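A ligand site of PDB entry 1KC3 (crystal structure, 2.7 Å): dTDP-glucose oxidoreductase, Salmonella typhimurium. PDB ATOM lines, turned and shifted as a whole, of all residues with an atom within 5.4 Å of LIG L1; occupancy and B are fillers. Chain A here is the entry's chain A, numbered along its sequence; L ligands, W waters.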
ATOM      1  N   THR A  65      21.512  -7.234  -4.389  1.00  0.00           N
ATOM      2  CA  THR A  65      21.574  -6.519  -3.088  1.00  0.00           C
ATOM      3  C   THR A  65      20.456  -6.903  -2.111  1.00  0.00           C
ATOM      4  O   THR A  65      20.188  -6.212  -1.109  1.00  0.00           O
ATOM      5  CB  THR A  65      21.513  -4.995  -3.343  1.00  0.00           C
ATOM      6  OG1 THR A  65      20.326  -4.686  -4.090  1.00  0.00           O
ATOM      7  CG2 THR A  65      22.577  -4.562  -4.252  1.00  0.00           C
ATOM      8  N   VAL A  67      19.977  -8.900   0.408  1.00  0.00           N
ATOM      9  CA  VAL A  67      20.923  -9.494   1.423  1.00  0.00           C
ATOM     10  C   VAL A  67      20.450 -10.813   2.119  1.00  0.00           C
ATOM     11  O   VAL A  67      21.204 -11.791   2.173  1.00  0.00           O
ATOM     12  CB  VAL A  67      21.335  -8.401   2.498  1.00  0.00           C
ATOM     13  CG1 VAL A  67      22.265  -8.945   3.566  1.00  0.00           C
ATOM     14  CG2 VAL A  67      22.019  -7.235   1.856  1.00  0.00           C
ATOM     15  N   ASP A  68      19.235 -10.792   2.684  1.00  0.00           N
ATOM     16  CA  ASP A  68      18.580 -11.965   3.355  1.00  0.00           C
ATOM     17  C   ASP A  68      18.195 -13.019   2.336  1.00  0.00           C
ATOM     18  O   ASP A  68      18.430 -14.217   2.568  1.00  0.00           O
ATOM     19  CB  ASP A  68      17.304 -11.639   4.130  1.00  0.00           C
ATOM     20  CG  ASP A  68      17.527 -10.687   5.286  1.00  0.00           C
ATOM     21  OD1 ASP A  68      18.543 -10.718   6.004  1.00  0.00           O
ATOM     22  OD2 ASP A  68      16.702  -9.800   5.560  1.00  0.00           O
ATOM     23  N   THR A 104      30.421  -3.040  -0.664  1.00  0.00           N
ATOM     24  CA  THR A 104      29.832  -2.871   0.653  1.00  0.00           C
ATOM     25  C   THR A 104      30.724  -3.035   1.854  1.00  0.00           C
ATOM     26  O   THR A 104      31.632  -3.783   1.821  1.00  0.00           O
ATOM     27  CB  THR A 104      28.749  -3.878   0.841  1.00  0.00           C
ATOM     28  OG1 THR A 104      28.293  -3.837   2.210  1.00  0.00           O
ATOM     29  CG2 THR A 104      29.255  -5.339   0.613  1.00  0.00           C
ATOM     30  N   ASP A 105      30.305  -2.394   2.937  1.00  0.00           N
ATOM     31  CA  ASP A 105      30.885  -2.568   4.266  1.00  0.00           C
ATOM     32  C   ASP A 105      30.579  -3.918   4.906  1.00  0.00           C
ATOM     33  O   ASP A 105      31.189  -4.291   5.903  1.00  0.00           O
ATOM     34  CB  ASP A 105      30.336  -1.524   5.214  1.00  0.00           C
ATOM     35  CG  ASP A 105      28.875  -1.806   5.674  1.00  0.00           C
ATOM     36  OD1 ASP A 105      27.899  -1.687   4.867  1.00  0.00           O
ATOM     37  OD2 ASP A 105      28.653  -2.151   6.858  1.00  0.00           O
ATOM     38  N   TYR A 106      29.598  -4.630   4.377  1.00  0.00           N
ATOM     39  CA  TYR A 106      29.245  -5.997   4.880  1.00  0.00           C
ATOM     40  C   TYR A 106      30.418  -7.025   4.637  1.00  0.00           C
ATOM     41  O   TYR A 106      30.435  -8.154   5.195  1.00  0.00           O
ATOM     42  CB  TYR A 106      27.837  -6.433   4.374  1.00  0.00           C
ATOM     43  CG  TYR A 106      26.643  -5.812   5.159  1.00  0.00           C
ATOM     44  CD1 TYR A 106      26.794  -4.616   5.903  1.00  0.00           C
ATOM     45  CD2 TYR A 106      25.375  -6.401   5.153  1.00  0.00           C
ATOM     46  CE1 TYR A 106      25.744  -4.019   6.616  1.00  0.00           C
ATOM     47  CE2 TYR A 106      24.289  -5.785   5.854  1.00  0.00           C
ATOM     48  CZ  TYR A 106      24.499  -4.589   6.591  1.00  0.00           C
ATOM     49  OH  TYR A 106      23.534  -3.912   7.322  1.00  0.00           O
ATOM     50  N   TYR A 128      25.955 -12.047   1.125  1.00  0.00           N
ATOM     51  CA  TYR A 128      26.019 -10.743   0.391  1.00  0.00           C
ATOM     52  C   TYR A 128      27.425 -10.117   0.340  1.00  0.00           C
ATOM     53  O   TYR A 128      27.936  -9.789  -0.714  1.00  0.00           O
ATOM     54  CB  TYR A 128      25.074  -9.701   1.028  1.00  0.00           C
ATOM     55  CG  TYR A 128      25.238  -8.309   0.432  1.00  0.00           C
ATOM     56  CD1 TYR A 128      24.976  -8.080  -0.921  1.00  0.00           C
ATOM     57  CD2 TYR A 128      25.666  -7.230   1.232  1.00  0.00           C
ATOM     58  CE1 TYR A 128      25.125  -6.823  -1.483  1.00  0.00           C
ATOM     59  CE2 TYR A 128      25.821  -5.982   0.690  1.00  0.00           C
ATOM     60  CZ  TYR A 128      25.569  -5.772  -0.675  1.00  0.00           C
ATOM     61  OH  TYR A 128      25.720  -4.509  -1.229  1.00  0.00           O
ATOM     62  N   THR A 151      30.490   1.392   0.176  1.00  0.00           N
ATOM     63  CA  THR A 151      29.564   2.287   0.803  1.00  0.00           C
ATOM     64  C   THR A 151      28.656   1.493   1.758  1.00  0.00           C
ATOM     65  O   THR A 151      28.808   0.259   1.961  1.00  0.00           O
ATOM     66  CB  THR A 151      28.817   3.082  -0.254  1.00  0.00           C
ATOM     67  OG1 THR A 151      28.097   4.143   0.385  1.00  0.00           O
ATOM     68  CG2 THR A 151      27.743   2.310  -0.971  1.00  0.00           C
ATOM     69  N   SER A 152      27.748   2.235   2.365  1.00  0.00           N
ATOM     70  CA  SER A 152      26.857   1.687   3.325  1.00  0.00           C
ATOM     71  C   SER A 152      25.620   2.480   3.546  1.00  0.00           C
ATOM     72  O   SER A 152      25.603   3.664   3.358  1.00  0.00           O
ATOM     73  CB  SER A 152      27.573   1.657   4.666  1.00  0.00           C
ATOM     74  OG  SER A 152      27.655   2.974   5.175  1.00  0.00           O
ATOM     75  N   TRP A 153      24.602   1.791   4.012  1.00  0.00           N
ATOM     76  CA  TRP A 153      23.267   2.328   4.413  1.00  0.00           C
ATOM     77  C   TRP A 153      22.792   3.346   3.381  1.00  0.00           C
ATOM     78  O   TRP A 153      22.605   4.544   3.663  1.00  0.00           O
ATOM     79  CB  TRP A 153      23.264   2.915   5.811  1.00  0.00           C
ATOM     80  CG  TRP A 153      23.650   1.926   6.932  1.00  0.00           C
ATOM     81  CD1 TRP A 153      24.202   0.678   6.824  1.00  0.00           C
ATOM     82  CD2 TRP A 153      23.551   2.180   8.327  1.00  0.00           C
ATOM     83  NE1 TRP A 153      24.423   0.156   8.071  1.00  0.00           N
ATOM     84  CE2 TRP A 153      24.038   1.063   9.011  1.00  0.00           C
ATOM     85  CE3 TRP A 153      23.089   3.266   9.076  1.00  0.00           C
ATOM     86  CZ2 TRP A 153      24.055   0.975  10.376  1.00  0.00           C
ATOM     87  CZ3 TRP A 153      23.135   3.188  10.442  1.00  0.00           C
ATOM     88  CH2 TRP A 153      23.603   2.054  11.078  1.00  0.00           C
ATOM     89  N   VAL A 154      22.641   2.797   2.161  1.00  0.00           N
ATOM     90  CA  VAL A 154      22.410   3.599   0.958  1.00  0.00           C
ATOM     91  C   VAL A 154      20.926   3.804   0.829  1.00  0.00           C
ATOM     92  O   VAL A 154      20.143   2.819   0.841  1.00  0.00           O
ATOM     93  CB  VAL A 154      23.114   2.967  -0.328  1.00  0.00           C
ATOM     94  CG1 VAL A 154      22.752   3.653  -1.644  1.00  0.00           C
ATOM     95  CG2 VAL A 154      24.613   2.991  -0.167  1.00  0.00           C
ATOM     96  N   PHE A 162      15.710   1.959   3.909  1.00  0.00           N
ATOM     97  CA  PHE A 162      15.331   1.968   5.322  1.00  0.00           C
ATOM     98  C   PHE A 162      14.386   3.121   5.701  1.00  0.00           C
ATOM     99  O   PHE A 162      13.378   2.873   6.323  1.00  0.00           O
ATOM    100  CB  PHE A 162      16.565   2.049   6.213  1.00  0.00           C
ATOM    101  CG  PHE A 162      16.273   2.067   7.703  1.00  0.00           C
ATOM    102  CD1 PHE A 162      16.112   0.877   8.405  1.00  0.00           C
ATOM    103  CD2 PHE A 162      16.227   3.273   8.405  1.00  0.00           C
ATOM    104  CE1 PHE A 162      15.897   0.904   9.775  1.00  0.00           C
ATOM    105  CE2 PHE A 162      16.015   3.305   9.797  1.00  0.00           C
ATOM    106  CZ  PHE A 162      15.848   2.118  10.472  1.00  0.00           C
ATOM    107  N   MET A 166      10.685   2.428   6.854  1.00  0.00           N
ATOM    108  CA  MET A 166      10.477   2.875   8.256  1.00  0.00           C
ATOM    109  C   MET A 166       9.315   3.857   8.420  1.00  0.00           C
ATOM    110  O   MET A 166       8.580   3.813   9.393  1.00  0.00           O
ATOM    111  CB  MET A 166      11.739   3.534   8.854  1.00  0.00           C
ATOM    112  CG  MET A 166      12.734   2.573   9.466  1.00  0.00           C
ATOM    113  SD  MET A 166      12.043   1.390  10.589  1.00  0.00           S
ATOM    114  CE  MET A 166      11.405   2.436  11.841  1.00  0.00           C
ATOM    115  N   SER A 177       8.817  -0.846  16.840  1.00  0.00           N
ATOM    116  CA  SER A 177      10.052  -1.497  17.383  1.00  0.00           C
ATOM    117  C   SER A 177      11.216  -1.755  16.421  1.00  0.00           C
ATOM    118  O   SER A 177      11.045  -2.535  15.482  1.00  0.00           O
ATOM    119  CB  SER A 177       9.719  -2.886  17.967  1.00  0.00           C
ATOM    120  OG  SER A 177       9.222  -3.770  16.976  1.00  0.00           O
ATOM    121  N   VAL A 178      12.390  -1.149  16.720  1.00  0.00           N
ATOM    122  CA  VAL A 178      13.686  -1.103  15.860  1.00  0.00           C
ATOM    123  C   VAL A 178      15.092  -1.005  16.603  1.00  0.00           C
ATOM    124  O   VAL A 178      15.168  -0.594  17.762  1.00  0.00           O
ATOM    125  CB  VAL A 178      13.633   0.073  14.826  1.00  0.00           C
ATOM    126  CG1 VAL A 178      14.938   0.291  13.980  1.00  0.00           C
ATOM    127  CG2 VAL A 178      12.489  -0.114  13.897  1.00  0.00           C
ATOM    128  N   ILE A 179      16.181  -1.361  15.897  1.00  0.00           N
ATOM    129  CA  ILE A 179      17.572  -1.443  16.401  1.00  0.00           C
ATOM    130  C   ILE A 179      18.400  -0.192  16.776  1.00  0.00           C
ATOM    131  O   ILE A 179      18.644   0.658  15.942  1.00  0.00           O
ATOM    132  CB  ILE A 179      18.445  -2.279  15.421  1.00  0.00           C
ATOM    133  CG1 ILE A 179      17.839  -3.674  15.258  1.00  0.00           C
ATOM    134  CG2 ILE A 179      19.952  -2.345  15.900  1.00  0.00           C
ATOM    135  CD1 ILE A 179      18.622  -4.642  14.447  1.00  0.00           C
ATOM    136  N   GLN A 182      23.510  -1.293  16.294  1.00  0.00           N
ATOM    137  CA  GLN A 182      24.251  -1.202  14.996  1.00  0.00           C
ATOM    138  C   GLN A 182      24.648   0.211  14.633  1.00  0.00           C
ATOM    139  O   GLN A 182      23.824   1.004  14.271  1.00  0.00           O
ATOM    140  CB  GLN A 182      23.486  -1.814  13.808  1.00  0.00           C
ATOM    141  CG  GLN A 182      23.739  -3.323  13.671  1.00  0.00           C
ATOM    142  CD  GLN A 182      23.129  -3.933  12.440  1.00  0.00           C
ATOM    143  OE1 GLN A 182      22.429  -4.926  12.542  1.00  0.00           O
ATOM    144  NE2 GLN A 182      23.400  -3.340  11.269  1.00  0.00           N
ATOM    145  N   TRP A 223      20.597   2.782  13.593  1.00  0.00           N
ATOM    146  CA  TRP A 223      19.334   2.602  12.838  1.00  0.00           C
ATOM    147  C   TRP A 223      18.144   3.216  13.629  1.00  0.00           C
ATOM    148  O   TRP A 223      17.233   3.813  13.020  1.00  0.00           O
ATOM    149  CB  TRP A 223      19.019   1.143  12.493  1.00  0.00           C
ATOM    150  CG  TRP A 223      19.908   0.487  11.469  1.00  0.00           C
ATOM    151  CD1 TRP A 223      20.806  -0.497  11.707  1.00  0.00           C
ATOM    152  CD2 TRP A 223      19.949   0.705  10.030  1.00  0.00           C
ATOM    153  NE1 TRP A 223      21.437  -0.873  10.543  1.00  0.00           N
ATOM    154  CE2 TRP A 223      20.931  -0.145   9.505  1.00  0.00           C
ATOM    155  CE3 TRP A 223      19.291   1.575   9.150  1.00  0.00           C
ATOM    156  CZ2 TRP A 223      21.250  -0.188   8.123  1.00  0.00           C
ATOM    157  CZ3 TRP A 223      19.621   1.547   7.782  1.00  0.00           C
ATOM    158  CH2 TRP A 223      20.592   0.677   7.286  1.00  0.00           C
ATOM    159  N   TYR A 254      15.603  -9.304  17.896  1.00  0.00           N
ATOM    160  CA  TYR A 254      14.809  -9.563  16.668  1.00  0.00           C
ATOM    161  C   TYR A 254      15.614 -10.219  15.496  1.00  0.00           C
ATOM    162  O   TYR A 254      16.546  -9.611  14.962  1.00  0.00           O
ATOM    163  CB  TYR A 254      14.008  -8.310  16.200  1.00  0.00           C
ATOM    164  CG  TYR A 254      12.675  -8.190  16.954  1.00  0.00           C
ATOM    165  CD1 TYR A 254      11.695  -9.224  16.883  1.00  0.00           C
ATOM    166  CD2 TYR A 254      12.405  -7.098  17.784  1.00  0.00           C
ATOM    167  CE1 TYR A 254      10.491  -9.151  17.625  1.00  0.00           C
ATOM    168  CE2 TYR A 254      11.181  -7.028  18.531  1.00  0.00           C
ATOM    169  CZ  TYR A 254      10.236  -8.055  18.437  1.00  0.00           C
ATOM    170  OH  TYR A 254       9.055  -7.996  19.136  1.00  0.00           O
ATOM    171  N   PRO A 255      15.226 -11.459  15.108  1.00  0.00           N
ATOM    172  CA  PRO A 255      15.871 -12.217  14.035  1.00  0.00           C
ATOM    173  C   PRO A 255      15.914 -11.660  12.643  1.00  0.00           C
ATOM    174  O   PRO A 255      14.965 -11.040  12.163  1.00  0.00           O
ATOM    175  CB  PRO A 255      14.976 -13.461  13.880  1.00  0.00           C
ATOM    176  CG  PRO A 255      14.119 -13.496  14.962  1.00  0.00           C
ATOM    177  CD  PRO A 255      14.117 -12.228  15.674  1.00  0.00           C
ATOM    178  N   ARG A 260      23.980  -9.539  10.322  1.00  0.00           N
ATOM    179  CA  ARG A 260      24.366  -8.150  10.083  1.00  0.00           C
ATOM    180  C   ARG A 260      25.602  -7.811  10.918  1.00  0.00           C
ATOM    181  O   ARG A 260      25.742  -8.334  12.030  1.00  0.00           O
ATOM    182  CB  ARG A 260      23.241  -7.158  10.429  1.00  0.00           C
ATOM    183  CG  ARG A 260      21.916  -7.326   9.630  1.00  0.00           C
ATOM    184  CD  ARG A 260      21.697  -6.353   8.455  1.00  0.00           C
ATOM    185  NE  ARG A 260      20.488  -6.711   7.685  1.00  0.00           N
ATOM    186  CZ  ARG A 260      20.360  -7.783   6.890  1.00  0.00           C
ATOM    187  NH1 ARG A 260      21.358  -8.634   6.674  1.00  0.00           N
ATOM    188  NH2 ARG A 260      19.206  -8.003   6.274  1.00  0.00           N
HETATM  189  O1  LIG L   1      19.023  -4.224   2.803  1.00  0.00           O
HETATM  190  P1  LIG L   1      19.675  -4.493   4.165  1.00  0.00           P
HETATM  191  O2  LIG L   1      20.388  -5.833   4.259  1.00  0.00           O
HETATM  192  O3  LIG L   1      20.729  -3.327   4.575  1.00  0.00           O
HETATM  193  C1  LIG L   1      22.020  -3.297   4.012  1.00  0.00           C
HETATM  194  C2  LIG L   1      22.685  -1.982   4.351  1.00  0.00           C
HETATM  195  O4  LIG L   1      22.075  -0.918   3.631  1.00  0.00           O
HETATM  196  C3  LIG L   1      24.140  -2.209   3.944  1.00  0.00           C
HETATM  197  O5  LIG L   1      24.969  -1.112   4.173  1.00  0.00           O
HETATM  198  C4  LIG L   1      24.229  -2.635   2.484  1.00  0.00           C
HETATM  199  O6  LIG L   1      25.644  -2.890   2.259  1.00  0.00           O
HETATM  200  C5  LIG L   1      23.249  -3.731   1.984  1.00  0.00           C
HETATM  201  O7  LIG L   1      21.981  -3.492   2.596  1.00  0.00           O
HETATM  202  C6  LIG L   1      22.898  -3.746   0.489  1.00  0.00           C
HETATM  203  O8  LIG L   1      18.665  -4.276   5.379  1.00  0.00           O
HETATM  204  P2  LIG L   1      17.810  -2.916   5.502  1.00  0.00           P
HETATM  205  O9  LIG L   1      16.514  -3.292   4.793  1.00  0.00           O
HETATM  206  O10 LIG L   1      18.659  -1.712   5.175  1.00  0.00           O
HETATM  207  O11 LIG L   1      17.478  -2.739   7.059  1.00  0.00           O
HETATM  208  C7  LIG L   1      18.376  -2.214   8.033  1.00  0.00           C
HETATM  209  C8  LIG L   1      17.731  -2.419   9.414  1.00  0.00           C
HETATM  210  O12 LIG L   1      16.278  -2.599   9.402  1.00  0.00           O
HETATM  211  C9  LIG L   1      18.211  -3.667  10.168  1.00  0.00           C
HETATM  212  O13 LIG L   1      19.508  -3.567  10.791  1.00  0.00           O
HETATM  213  C10 LIG L   1      17.083  -3.811  11.170  1.00  0.00           C
HETATM  214  C11 LIG L   1      15.926  -2.886  10.745  1.00  0.00           C
HETATM  215  N1  LIG L   1      14.712  -3.649  11.161  1.00  0.00           N
HETATM  216  C12 LIG L   1      14.137  -3.341  12.350  1.00  0.00           C
HETATM  217  O14 LIG L   1      14.541  -2.416  13.031  1.00  0.00           O
HETATM  218  N2  LIG L   1      13.100  -4.006  12.888  1.00  0.00           N
HETATM  219  C13 LIG L   1      12.569  -5.085  12.279  1.00  0.00           C
HETATM  220  O15 LIG L   1      11.598  -5.693  12.778  1.00  0.00           O
HETATM  221  C14 LIG L   1      13.184  -5.481  10.978  1.00  0.00           C
HETATM  222  C15 LIG L   1      12.645  -6.683  10.250  1.00  0.00           C
HETATM  223  C16 LIG L   1      14.267  -4.723  10.475  1.00  0.00           C
HETATM  224  P1  LG2 L   2      19.634  -1.143  -5.857  1.00  0.00           P
HETATM  225  O1  LG2 L   2      19.025  -2.484  -5.468  1.00  0.00           O
HETATM  226  O2  LG2 L   2      18.688   0.034  -5.848  1.00  0.00           O
HETATM  227  O3  LG2 L   2      20.357  -1.352  -7.296  1.00  0.00           O
HETATM  228  C1  LG2 L   2      20.952  -2.521  -7.822  1.00  0.00           C
HETATM  229  C2  LG2 L   2      20.485  -2.773  -9.255  1.00  0.00           C
HETATM  230  O4  LG2 L   2      20.734  -4.093  -9.715  1.00  0.00           O
HETATM  231  C3  LG2 L   2      18.983  -2.587  -9.432  1.00  0.00           C
HETATM  232  O5  LG2 L   2      18.776  -1.743 -10.542  1.00  0.00           O
HETATM  233  C4  LG2 L   2      18.455  -3.959  -9.698  1.00  0.00           C
HETATM  234  O6  LG2 L   2      17.109  -3.895 -10.243  1.00  0.00           O
HETATM  235  C5  LG2 L   2      19.564  -4.472 -10.511  1.00  0.00           C
HETATM  236  N1  LG2 L   2      19.481  -5.885 -10.708  1.00  0.00           N
HETATM  237  C6  LG2 L   2      18.892  -6.889  -9.948  1.00  0.00           C
HETATM  238  N2  LG2 L   2      19.072  -8.046 -10.574  1.00  0.00           N
HETATM  239  C7  LG2 L   2      19.753  -7.783 -11.696  1.00  0.00           C
HETATM  240  C8  LG2 L   2      20.215  -8.614 -12.705  1.00  0.00           C
HETATM  241  N3  LG2 L   2      20.029  -9.991 -12.780  1.00  0.00           N
HETATM  242  N4  LG2 L   2      20.886  -8.011 -13.741  1.00  0.00           N
HETATM  243  C9  LG2 L   2      21.138  -6.639 -13.798  1.00  0.00           C
HETATM  244  N5  LG2 L   2      20.694  -5.811 -12.800  1.00  0.00           N
HETATM  245  C10 LG2 L   2      20.010  -6.421 -11.784  1.00  0.00           C
HETATM  246  O7  LG2 L   2      20.929  -1.023  -4.991  1.00  0.00           O
HETATM  247  P2  LG2 L   2      21.659   0.378  -4.820  1.00  0.00           P
HETATM  248  O8  LG2 L   2      21.518   1.336  -5.978  1.00  0.00           O
HETATM  249  O9  LG2 L   2      21.430   0.831  -3.368  1.00  0.00           O
HETATM  250  O10 LG2 L   2      23.236   0.065  -4.767  1.00  0.00           O
HETATM  251  C11 LG2 L   2      24.062   0.206  -5.919  1.00  0.00           C
HETATM  252  C12 LG2 L   2      25.446  -0.336  -5.763  1.00  0.00           C
HETATM  253  O11 LG2 L   2      25.879  -0.010  -4.440  1.00  0.00           O
HETATM  254  C13 LG2 L   2      25.592  -1.869  -5.937  1.00  0.00           C
HETATM  255  O12 LG2 L   2      26.853  -2.327  -6.292  1.00  0.00           O
HETATM  256  C14 LG2 L   2      25.410  -2.328  -4.548  1.00  0.00           C
HETATM  257  O13 LG2 L   2      25.898  -3.583  -4.190  1.00  0.00           O
HETATM  258  C15 LG2 L   2      26.160  -1.236  -3.827  1.00  0.00           C
HETATM  259  N6  LG2 L   2      25.702  -1.133  -2.379  1.00  0.00           N
HETATM  260  C16 LG2 L   2      24.366  -0.778  -1.959  1.00  0.00           C
HETATM  261  C17 LG2 L   2      23.955  -0.670  -0.674  1.00  0.00           C
HETATM  262  C18 LG2 L   2      22.595  -0.313  -0.124  1.00  0.00           C
HETATM  263  O14 LG2 L   2      22.433   0.053   1.056  1.00  0.00           O
HETATM  264  N7  LG2 L   2      21.505  -0.357  -0.942  1.00  0.00           N
HETATM  265  C19 LG2 L   2      25.109  -0.651   0.287  1.00  0.00           C
HETATM  266  C20 LG2 L   2      26.385  -1.326  -0.099  1.00  0.00           C
HETATM  267  C21 LG2 L   2      26.645  -1.394  -1.389  1.00  0.00           C
HETATM  268  P3  LG2 L   2      15.706  -4.698  -9.867  1.00  0.00           P
HETATM  269  O15 LG2 L   2      14.720  -3.601  -9.478  1.00  0.00           O
HETATM  270  O16 LG2 L   2      15.958  -5.629  -8.703  1.00  0.00           O
HETATM  271  O17 LG2 L   2      15.367  -5.450 -11.137  1.00  0.00           O
HETATM  272  O   HOH W   1      16.517  -1.165   2.797  1.00  0.00           O
HETATM  273  O   HOH W   2      20.074  -5.906  11.974  1.00  0.00           O
HETATM  274  O   HOH W   3      19.545  -0.119   3.362  1.00  0.00           O
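The side-chain hydroxyl (OG1) of Thr 104 is in hydrogen-bond range of an oxygen (O6) of LIG L1, 2.8 Å away.
N of Trp 153 is in hydrogen-bond range of O5 of LIG L1, at 2.9 Å.
The side-chain carboxylate (OD1) of Asp 105 sits at hydrogen-bond distance from an oxygen (O5) of LIG L1 (3.1 Å).
The guanidinium group (NH2) of Arg 260 is in salt-bridge range of an oxygen (O2) of LIG L1 (3.2 Å).
NE1 of Trp 223 sits at hydrogen-bond distance from O13 of LIG L1 (3.3 Å).
N of Ile 179 sits at hydrogen-bond distance from O14 of LIG L1, at 3.5 Å.
OH of Tyr 128 sits at hydrogen-bond distance from O13 of LG2 L2, at 3.1 Å.
An oxygen (O1) of LG2 L2 sits at hydrogen-bond distance from the side-chain hydroxyl (OG1) of Thr 65 (2.9 Å).
The backbone NH of Val 154 lies within hydrogen-bond range of an oxygen (O14) of LG2 L2, at 3.0 Å.
An oxygen (O14) of LG2 L2 is in hydrogen-bond range of an oxygen (O4) of LIG L1 (2.8 Å).
OD1 of Asp 105 sits at hydrogen-bond distance from OG1 of Thr 104.
N of Tyr 106 sits at hydrogen-bond distance from OG1 of Thr 104, at 2.7 Å.
The backbone NH (N) of Asp 105 lies within hydrogen-bond range of the backbone carbonyl oxygen (O) of Thr 151, at 3.2 Å.
NH2 of Arg 260 is in salt-bridge range of OD1 of Asp 68.
The indole nitrogen of Trp 223 sits close to the side-chain amide nitrogen of Gln 182 (3.2 Å).
O of Thr 65 touches C6 of LIG L1 (3.997 Å).
Val 67 touches LIG L1 (CG2 to O2, 3.2 Å).
Tyr 106 touches LIG L1 (CZ to C3, 3.6 Å).
Tyr 128 touches LIG L1.
Ser 152 touches LIG L1 (CA to O5, 3.5 Å).
Phe 162 touches LIG L1 (CE1 to O12, 3.5 Å).
Ser 177 touches LIG L1.
Val 178 touches LIG L1 (CG1 to O14, 2.9 Å).
OE1 of Gln 182 touches O13 of LIG L1, 3.7 Å away.
Of the 21 residues printed, 15 come within 4 Å of LIG L1.
The nearest printed residue that does not touch LIG L1 is Val 154 (4.04 Å).
Water W2 bridges the side-chain amide oxygen of Gln 182 and an oxygen (O13) of LIG L1.
Water W1 bridges O9 of LIG L1 and N of Phe 162.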
